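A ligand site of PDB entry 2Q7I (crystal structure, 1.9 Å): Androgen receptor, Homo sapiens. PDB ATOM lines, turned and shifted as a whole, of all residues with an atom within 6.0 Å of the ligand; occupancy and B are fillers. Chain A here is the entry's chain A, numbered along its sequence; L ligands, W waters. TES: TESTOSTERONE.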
ATOM      1  N   LEU A  39      -3.904 -16.588  29.636  1.00  0.00           N
ATOM      2  CA  LEU A  39      -2.794 -17.476  29.315  1.00  0.00           C
ATOM      3  C   LEU A  39      -2.420 -18.373  30.489  1.00  0.00           C
ATOM      4  O   LEU A  39      -2.098 -19.521  30.292  1.00  0.00           O
ATOM      5  CB  LEU A  39      -1.579 -16.717  28.796  1.00  0.00           C
ATOM      6  CG  LEU A  39      -1.505 -16.522  27.281  1.00  0.00           C
ATOM      7  CD1 LEU A  39      -1.246 -17.865  26.582  1.00  0.00           C
ATOM      8  CD2 LEU A  39      -2.758 -15.857  26.710  1.00  0.00           C
ATOM      9  N   LEU A  42      -5.021 -21.065  30.364  1.00  0.00           N
ATOM     10  CA  LEU A  42      -4.706 -21.995  29.280  1.00  0.00           C
ATOM     11  C   LEU A  42      -3.585 -22.952  29.675  1.00  0.00           C
ATOM     12  O   LEU A  42      -3.636 -24.158  29.365  1.00  0.00           O
ATOM     13  CB  LEU A  42      -4.325 -21.255  27.993  1.00  0.00           C
ATOM     14  CG  LEU A  42      -5.473 -20.631  27.192  1.00  0.00           C
ATOM     15  CD1 LEU A  42      -4.890 -19.766  26.087  1.00  0.00           C
ATOM     16  CD2 LEU A  42      -6.404 -21.687  26.589  1.00  0.00           C
ATOM     17  N   ASN A  43      -2.576 -22.426  30.360  1.00  0.00           N
ATOM     18  CA  ASN A  43      -1.453 -23.231  30.828  1.00  0.00           C
ATOM     19  C   ASN A  43      -1.891 -24.286  31.852  1.00  0.00           C
ATOM     20  O   ASN A  43      -1.439 -25.446  31.796  1.00  0.00           O
ATOM     21  CB  ASN A  43      -0.359 -22.348  31.440  1.00  0.00           C
ATOM     22  CG  ASN A  43       0.402 -21.537  30.383  1.00  0.00           C
ATOM     23  OD1 ASN A  43       0.376 -21.839  29.192  1.00  0.00           O
ATOM     24  ND2 ASN A  43       1.113 -20.500  30.843  1.00  0.00           N
ATOM     25  N   LEU A  45      -4.913 -25.483  32.089  1.00  0.00           N
ATOM     26  CA  LEU A  45      -5.725 -26.412  31.300  1.00  0.00           C
ATOM     27  C   LEU A  45      -4.848 -27.440  30.601  1.00  0.00           C
ATOM     28  O   LEU A  45      -5.149 -28.630  30.588  1.00  0.00           O
ATOM     29  CB  LEU A  45      -6.587 -25.662  30.271  1.00  0.00           C
ATOM     30  CG  LEU A  45      -7.505 -26.569  29.428  1.00  0.00           C
ATOM     31  CD1 LEU A  45      -8.500 -27.339  30.311  1.00  0.00           C
ATOM     32  CD2 LEU A  45      -8.237 -25.805  28.339  1.00  0.00           C
ATOM     33  N   GLY A  46      -3.742 -26.983  30.018  1.00  0.00           N
ATOM     34  CA  GLY A  46      -2.753 -27.883  29.422  1.00  0.00           C
ATOM     35  C   GLY A  46      -2.205 -28.898  30.419  1.00  0.00           C
ATOM     36  O   GLY A  46      -2.084 -30.071  30.106  1.00  0.00           O
ATOM     37  N   GLN A  49      -5.075 -31.388  31.121  1.00  0.00           N
ATOM     38  CA  GLN A  49      -5.299 -32.240  29.952  1.00  0.00           C
ATOM     39  C   GLN A  49      -4.154 -33.217  29.733  1.00  0.00           C
ATOM     40  O   GLN A  49      -4.379 -34.320  29.249  1.00  0.00           O
ATOM     41  CB  GLN A  49      -5.531 -31.413  28.677  1.00  0.00           C
ATOM     42  CG  GLN A  49      -6.922 -30.787  28.655  1.00  0.00           C
ATOM     43  CD  GLN A  49      -7.359 -30.243  27.302  1.00  0.00           C
ATOM     44  OE1 GLN A  49      -8.354 -29.498  27.212  1.00  0.00           O
ATOM     45  NE2 GLN A  49      -6.648 -30.599  26.249  1.00  0.00           N
ATOM     46  N   TRP A  79       1.522 -33.742  22.188  1.00  0.00           N
ATOM     47  CA  TRP A  79       0.406 -33.215  22.998  1.00  0.00           C
ATOM     48  C   TRP A  79      -0.244 -31.971  22.419  1.00  0.00           C
ATOM     49  O   TRP A  79      -1.462 -31.847  22.457  1.00  0.00           O
ATOM     50  CB  TRP A  79       0.807 -32.944  24.453  1.00  0.00           C
ATOM     51  CG  TRP A  79       1.910 -31.989  24.603  1.00  0.00           C
ATOM     52  CD1 TRP A  79       3.240 -32.284  24.565  1.00  0.00           C
ATOM     53  CD2 TRP A  79       1.824 -30.568  24.811  1.00  0.00           C
ATOM     54  NE1 TRP A  79       3.987 -31.144  24.725  1.00  0.00           N
ATOM     55  CE2 TRP A  79       3.140 -30.085  24.879  1.00  0.00           C
ATOM     56  CE3 TRP A  79       0.760 -29.671  24.935  1.00  0.00           C
ATOM     57  CZ2 TRP A  79       3.432 -28.728  25.078  1.00  0.00           C
ATOM     58  CZ3 TRP A  79       1.034 -28.328  25.132  1.00  0.00           C
ATOM     59  CH2 TRP A  79       2.358 -27.861  25.188  1.00  0.00           C
ATOM     60  N   MET A  80       0.562 -31.049  21.881  1.00  0.00           N
ATOM     61  CA  MET A  80      -0.008 -29.805  21.343  1.00  0.00           C
ATOM     62  C   MET A  80      -0.996 -30.102  20.220  1.00  0.00           C
ATOM     63  O   MET A  80      -2.124 -29.606  20.246  1.00  0.00           O
ATOM     64  CB  MET A  80       1.087 -28.842  20.870  1.00  0.00           C
ATOM     65  CG  MET A  80       0.561 -27.500  20.391  1.00  0.00           C
ATOM     66  SD  MET A  80       0.039 -26.421  21.729  1.00  0.00           S
ATOM     67  CE  MET A  80       1.661 -25.948  22.321  1.00  0.00           C
ATOM     68  N   MET A  83      -4.163 -31.984  21.490  1.00  0.00           N
ATOM     69  CA  MET A  83      -5.052 -31.111  22.253  1.00  0.00           C
ATOM     70  C   MET A  83      -5.760 -30.072  21.379  1.00  0.00           C
ATOM     71  O   MET A  83      -6.923 -29.771  21.606  1.00  0.00           O
ATOM     72  CB  MET A  83      -4.279 -30.411  23.367  1.00  0.00           C
ATOM     73  CG  MET A  83      -3.838 -31.375  24.496  1.00  0.00           C
ATOM     74  SD  MET A  83      -2.943 -30.532  25.784  1.00  0.00           S
ATOM     75  CE  MET A  83      -2.459 -31.940  26.805  1.00  0.00           C
ATOM     76  N   VAL A  84      -5.048 -29.527  20.403  1.00  0.00           N
ATOM     77  CA  VAL A  84      -5.648 -28.590  19.447  1.00  0.00           C
ATOM     78  C   VAL A  84      -6.745 -29.279  18.619  1.00  0.00           C
ATOM     79  O   VAL A  84      -7.833 -28.729  18.403  1.00  0.00           O
ATOM     80  CB  VAL A  84      -4.564 -28.019  18.499  1.00  0.00           C
ATOM     81  CG1 VAL A  84      -5.201 -27.373  17.247  1.00  0.00           C
ATOM     82  CG2 VAL A  84      -3.715 -27.035  19.234  1.00  0.00           C
ATOM     83  N   MET A  87      -9.715 -29.908  20.767  1.00  0.00           N
ATOM     84  CA  MET A  87     -10.375 -28.630  21.047  1.00  0.00           C
ATOM     85  C   MET A  87     -11.204 -28.196  19.836  1.00  0.00           C
ATOM     86  O   MET A  87     -12.352 -27.748  19.987  1.00  0.00           O
ATOM     87  CB  MET A  87      -9.330 -27.567  21.411  1.00  0.00           C
ATOM     88  CG  MET A  87      -9.926 -26.248  21.879  1.00  0.00           C
ATOM     89  SD  MET A  87     -10.379 -25.115  20.552  1.00  0.00           S
ATOM     90  CE  MET A  87      -8.767 -24.683  19.943  1.00  0.00           C
ATOM     91  N   ARG A  90     -14.371 -30.227  19.900  1.00  0.00           N
ATOM     92  CA  ARG A  90     -15.279 -29.684  20.935  1.00  0.00           C
ATOM     93  C   ARG A  90     -15.934 -28.397  20.475  1.00  0.00           C
ATOM     94  O   ARG A  90     -17.127 -28.177  20.723  1.00  0.00           O
ATOM     95  CB  ARG A  90     -14.528 -29.387  22.242  1.00  0.00           C
ATOM     96  CG  ARG A  90     -14.086 -30.599  22.976  1.00  0.00           C
ATOM     97  CD  ARG A  90     -13.683 -30.268  24.402  1.00  0.00           C
ATOM     98  NE  ARG A  90     -12.556 -29.330  24.489  1.00  0.00           N
ATOM     99  CZ  ARG A  90     -11.270 -29.667  24.376  1.00  0.00           C
ATOM    100  NH1 ARG A  90     -10.894 -30.922  24.154  1.00  0.00           N
ATOM    101  NH2 ARG A  90     -10.348 -28.733  24.510  1.00  0.00           N
ATOM    102  N   TYR A 101     -13.802 -23.583  22.076  1.00  0.00           N
ATOM    103  CA  TYR A 101     -14.238 -24.221  23.301  1.00  0.00           C
ATOM    104  C   TYR A 101     -13.065 -24.948  23.969  1.00  0.00           C
ATOM    105  O   TYR A 101     -12.965 -26.179  23.924  1.00  0.00           O
ATOM    106  CB  TYR A 101     -15.391 -25.182  22.965  1.00  0.00           C
ATOM    107  CG  TYR A 101     -16.254 -25.618  24.119  1.00  0.00           C
ATOM    108  CD1 TYR A 101     -15.870 -26.689  24.932  1.00  0.00           C
ATOM    109  CD2 TYR A 101     -17.473 -25.009  24.385  1.00  0.00           C
ATOM    110  CE1 TYR A 101     -16.670 -27.113  25.980  1.00  0.00           C
ATOM    111  CE2 TYR A 101     -18.289 -25.438  25.451  1.00  0.00           C
ATOM    112  CZ  TYR A 101     -17.876 -26.492  26.238  1.00  0.00           C
ATOM    113  OH  TYR A 101     -18.641 -26.954  27.286  1.00  0.00           O
ATOM    114  N   PHE A 102     -12.170 -24.181  24.583  1.00  0.00           N
ATOM    115  CA  PHE A 102     -11.003 -24.780  25.241  1.00  0.00           C
ATOM    116  C   PHE A 102     -11.467 -25.668  26.393  1.00  0.00           C
ATOM    117  O   PHE A 102     -10.982 -26.781  26.560  1.00  0.00           O
ATOM    118  CB  PHE A 102     -10.047 -23.708  25.754  1.00  0.00           C
ATOM    119  CG  PHE A 102      -9.285 -22.993  24.673  1.00  0.00           C
ATOM    120  CD1 PHE A 102      -8.192 -23.593  24.077  1.00  0.00           C
ATOM    121  CD2 PHE A 102      -9.641 -21.723  24.279  1.00  0.00           C
ATOM    122  CE1 PHE A 102      -7.478 -22.950  23.080  1.00  0.00           C
ATOM    123  CE2 PHE A 102      -8.929 -21.057  23.291  1.00  0.00           C
ATOM    124  CZ  PHE A 102      -7.847 -21.664  22.690  1.00  0.00           C
ATOM    125  N   ALA A 103     -12.415 -25.141  27.162  1.00  0.00           N
ATOM    126  CA  ALA A 103     -13.048 -25.871  28.242  1.00  0.00           C
ATOM    127  C   ALA A 103     -14.416 -25.238  28.517  1.00  0.00           C
ATOM    128  O   ALA A 103     -14.689 -24.126  28.036  1.00  0.00           O
ATOM    129  CB  ALA A 103     -12.172 -25.820  29.473  1.00  0.00           C
ATOM    130  N   MET A 118      -2.988 -14.069  20.612  1.00  0.00           N
ATOM    131  CA  MET A 118      -2.866 -15.250  19.770  1.00  0.00           C
ATOM    132  C   MET A 118      -3.909 -15.247  18.675  1.00  0.00           C
ATOM    133  O   MET A 118      -4.352 -16.316  18.252  1.00  0.00           O
ATOM    134  CB  MET A 118      -3.083 -16.512  20.606  1.00  0.00           C
ATOM    135  CG  MET A 118      -1.968 -16.832  21.536  1.00  0.00           C
ATOM    136  SD  MET A 118      -2.124 -18.528  22.123  1.00  0.00           S
ATOM    137  CE  MET A 118      -3.602 -18.407  23.113  1.00  0.00           C
ATOM    138  N   MET A 125      -7.034 -22.154  14.280  1.00  0.00           N
ATOM    139  CA  MET A 125      -7.710 -23.190  15.057  1.00  0.00           C
ATOM    140  C   MET A 125      -9.214 -23.215  14.797  1.00  0.00           C
ATOM    141  O   MET A 125      -9.812 -24.288  14.730  1.00  0.00           O
ATOM    142  CB  MET A 125      -7.434 -23.042  16.558  1.00  0.00           C
ATOM    143  CG  MET A 125      -6.007 -23.405  16.934  1.00  0.00           C
ATOM    144  SD  MET A 125      -5.724 -23.503  18.709  1.00  0.00           S
ATOM    145  CE  MET A 125      -5.508 -21.808  19.184  1.00  0.00           C
ATOM    146  N   LEU A 211       2.000 -22.584  17.695  1.00  0.00           N
ATOM    147  CA  LEU A 211       1.737 -22.593  19.122  1.00  0.00           C
ATOM    148  C   LEU A 211       2.973 -22.984  19.938  1.00  0.00           C
ATOM    149  O   LEU A 211       3.226 -22.391  20.988  1.00  0.00           O
ATOM    150  CB  LEU A 211       0.535 -23.499  19.440  1.00  0.00           C
ATOM    151  CG  LEU A 211      -0.800 -22.997  18.899  1.00  0.00           C
ATOM    152  CD1 LEU A 211      -1.868 -24.066  19.052  1.00  0.00           C
ATOM    153  CD2 LEU A 211      -1.246 -21.703  19.577  1.00  0.00           C
ATOM    154  N   PHE A 214       5.026 -19.862  20.046  1.00  0.00           N
ATOM    155  CA  PHE A 214       4.377 -18.869  20.921  1.00  0.00           C
ATOM    156  C   PHE A 214       4.577 -19.190  22.403  1.00  0.00           C
ATOM    157  O   PHE A 214       4.974 -18.316  23.196  1.00  0.00           O
ATOM    158  CB  PHE A 214       2.896 -18.763  20.572  1.00  0.00           C
ATOM    159  CG  PHE A 214       2.182 -17.692  21.348  1.00  0.00           C
ATOM    160  CD1 PHE A 214       1.717 -17.928  22.635  1.00  0.00           C
ATOM    161  CD2 PHE A 214       2.005 -16.422  20.797  1.00  0.00           C
ATOM    162  CE1 PHE A 214       1.058 -16.930  23.360  1.00  0.00           C
ATOM    163  CE2 PHE A 214       1.353 -15.418  21.519  1.00  0.00           C
ATOM    164  CZ  PHE A 214       0.872 -15.676  22.793  1.00  0.00           C
ATOM    165  N   THR A 215       4.302 -20.434  22.779  1.00  0.00           N
ATOM    166  CA  THR A 215       4.402 -20.852  24.183  1.00  0.00           C
ATOM    167  C   THR A 215       5.860 -20.868  24.665  1.00  0.00           C
ATOM    168  O   THR A 215       6.130 -20.520  25.819  1.00  0.00           O
ATOM    169  CB  THR A 215       3.701 -22.215  24.432  1.00  0.00           C
ATOM    170  OG1 THR A 215       3.450 -22.378  25.835  1.00  0.00           O
ATOM    171  CG2 THR A 215       4.521 -23.402  23.928  1.00  0.00           C
ATOM    172  N   LEU A 218       6.779 -17.312  25.282  1.00  0.00           N
ATOM    173  CA  LEU A 218       6.053 -16.874  26.476  1.00  0.00           C
ATOM    174  C   LEU A 218       6.694 -17.395  27.758  1.00  0.00           C
ATOM    175  O   LEU A 218       6.831 -16.655  28.736  1.00  0.00           O
ATOM    176  CB  LEU A 218       4.594 -17.322  26.392  1.00  0.00           C
ATOM    177  CG  LEU A 218       3.657 -16.861  27.503  1.00  0.00           C
ATOM    178  CD1 LEU A 218       3.715 -15.340  27.713  1.00  0.00           C
ATOM    179  CD2 LEU A 218       2.250 -17.293  27.162  1.00  0.00           C
ATOM    180  N   PHE A 229       3.252 -20.721  34.505  1.00  0.00           N
ATOM    181  CA  PHE A 229       3.357 -22.046  33.873  1.00  0.00           C
ATOM    182  C   PHE A 229       3.448 -23.094  34.969  1.00  0.00           C
ATOM    183  O   PHE A 229       4.332 -23.004  35.818  1.00  0.00           O
ATOM    184  CB  PHE A 229       4.607 -22.140  32.993  1.00  0.00           C
ATOM    185  CG  PHE A 229       4.450 -21.506  31.638  1.00  0.00           C
ATOM    186  CD1 PHE A 229       4.631 -20.122  31.488  1.00  0.00           C
ATOM    187  CD2 PHE A 229       4.171 -22.270  30.517  1.00  0.00           C
ATOM    188  CE1 PHE A 229       4.500 -19.520  30.234  1.00  0.00           C
ATOM    189  CE2 PHE A 229       4.039 -21.682  29.265  1.00  0.00           C
ATOM    190  CZ  PHE A 229       4.200 -20.303  29.125  1.00  0.00           C
ATOM    191  N   MET A 233       4.185 -28.386  32.263  1.00  0.00           N
ATOM    192  CA  MET A 233       4.210 -27.489  31.097  1.00  0.00           C
ATOM    193  C   MET A 233       5.578 -26.826  30.971  1.00  0.00           C
ATOM    194  O   MET A 233       6.176 -26.855  29.915  1.00  0.00           O
ATOM    195  CB  MET A 233       3.098 -26.443  31.196  1.00  0.00           C
ATOM    196  CG  MET A 233       1.696 -27.028  31.066  1.00  0.00           C
ATOM    197  SD  MET A 233       1.378 -27.820  29.471  1.00  0.00           S
ATOM    198  CE  MET A 233       0.933 -26.395  28.497  1.00  0.00           C
ATOM    199  N   ILE A 237       8.005 -27.685  27.902  1.00  0.00           N
ATOM    200  CA  ILE A 237       8.227 -26.587  26.959  1.00  0.00           C
ATOM    201  C   ILE A 237       9.711 -26.159  26.891  1.00  0.00           C
ATOM    202  O   ILE A 237      10.147 -25.638  25.875  1.00  0.00           O
ATOM    203  CB  ILE A 237       7.283 -25.396  27.265  1.00  0.00           C
ATOM    204  CG1 ILE A 237       5.832 -25.799  26.974  1.00  0.00           C
ATOM    205  CG2 ILE A 237       7.655 -24.166  26.417  1.00  0.00           C
ATOM    206  CD1 ILE A 237       4.782 -24.908  27.576  1.00  0.00           C
HETATM  207  C1  TES L   1      -4.688 -26.280  26.248  1.00  0.00           C
HETATM  208  C2  TES L   1      -5.680 -27.400  25.966  1.00  0.00           C
HETATM  209  C3  TES L   1      -6.451 -27.090  24.707  1.00  0.00           C
HETATM  210  O3  TES L   1      -7.600 -27.504  24.579  1.00  0.00           O
HETATM  211  C4  TES L   1      -5.815 -26.286  23.651  1.00  0.00           C
HETATM  212  C5  TES L   1      -4.583 -25.746  23.796  1.00  0.00           C
HETATM  213  C6  TES L   1      -3.985 -24.996  22.630  1.00  0.00           C
HETATM  214  C7  TES L   1      -3.343 -23.691  23.095  1.00  0.00           C
HETATM  215  C8  TES L   1      -2.326 -23.963  24.196  1.00  0.00           C
HETATM  216  C9  TES L   1      -2.984 -24.654  25.405  1.00  0.00           C
HETATM  217  C10 TES L   1      -3.768 -25.944  25.056  1.00  0.00           C
HETATM  218  C11 TES L   1      -1.955 -24.859  26.537  1.00  0.00           C
HETATM  219  C12 TES L   1      -1.245 -23.573  26.930  1.00  0.00           C
HETATM  220  C13 TES L   1      -0.584 -22.895  25.732  1.00  0.00           C
HETATM  221  C14 TES L   1      -1.635 -22.669  24.652  1.00  0.00           C
HETATM  222  C15 TES L   1      -0.902 -21.795  23.622  1.00  0.00           C
HETATM  223  C16 TES L   1      -0.031 -20.867  24.495  1.00  0.00           C
HETATM  224  C17 TES L   1      -0.110 -21.444  25.917  1.00  0.00           C
HETATM  225  O17 TES L   1       1.128 -21.308  26.604  1.00  0.00           O
HETATM  226  C18 TES L   1       0.583 -23.777  25.253  1.00  0.00           C
HETATM  227  C19 TES L   1      -2.858 -27.147  24.745  1.00  0.00           C
HETATM  228  O   HOH W   1      -7.963 -30.594  23.999  1.00  0.00           O
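OG1 of Thr 215 lies within hydrogen-bond range of O17 of the ligand.
An oxygen (O17) of the ligand is in hydrogen-bond range of the side-chain amide oxygen (OD1) of Asn 43, at 2.7 Å.
The guanidinium group of Arg 90 lies within hydrogen-bond range of an oxygen (O3) of the ligand (3.0 Å).
The side-chain amide oxygen of Gln 49 lies close to an oxygen (O3) of the ligand, at 3.4 Å.
The backbone carbonyl oxygen (O) of Leu 39 lies close to the side-chain amide nitrogen (ND2) of Asn 43, 3.4 Å away.
OE1 of Gln 49 lies within hydrogen-bond range of NH2 of Arg 90 (3.4 Å).
The backbone carbonyl oxygen of Phe 102 lies within hydrogen-bond range of the guanidinium group of Arg 90.
NE of Arg 90 sits at hydrogen-bond distance from O of Tyr 101, at 3.2 Å.
The side-chain amide nitrogen of Gln 49 sits close to the side-chain sulfur of Met 83, 3.7 Å away.
Leu 39 touches the ligand (CD1 to C17, 3.8 Å).
O of Leu 42 touches C11 of the ligand (3.4 Å).
Leu 45 touches the ligand (CD2 to C2, 3.8 Å).
Gly 46 touches the ligand.
Met 80 touches the ligand.
Met 83 touches the ligand.
CG2 of Val 84 touches C6 of the ligand, 3.97 Å away.
Met 87 touches the ligand.
CD1 of Phe 102 touches C4 of the ligand (3.6 Å).
SD of Met 118 touches C15 of the ligand, 3.8 Å away.
Phe 214 touches the ligand (CD1 to C16, 3.9 Å).
Phe 229 touches the ligand.
Met 233 touches the ligand (CE to C11, 3.8 Å).
Along chain A the residues within 4 Å of the ligand span positions 39 to 233.
The nearest printed residue that does not touch the ligand is Leu 211 (4.1 Å).
Water W1 lies within hydrogen-bond range of NE2 of Gln 49, O of Met 83, NH1 of Arg 90 and O3 of the ligand.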
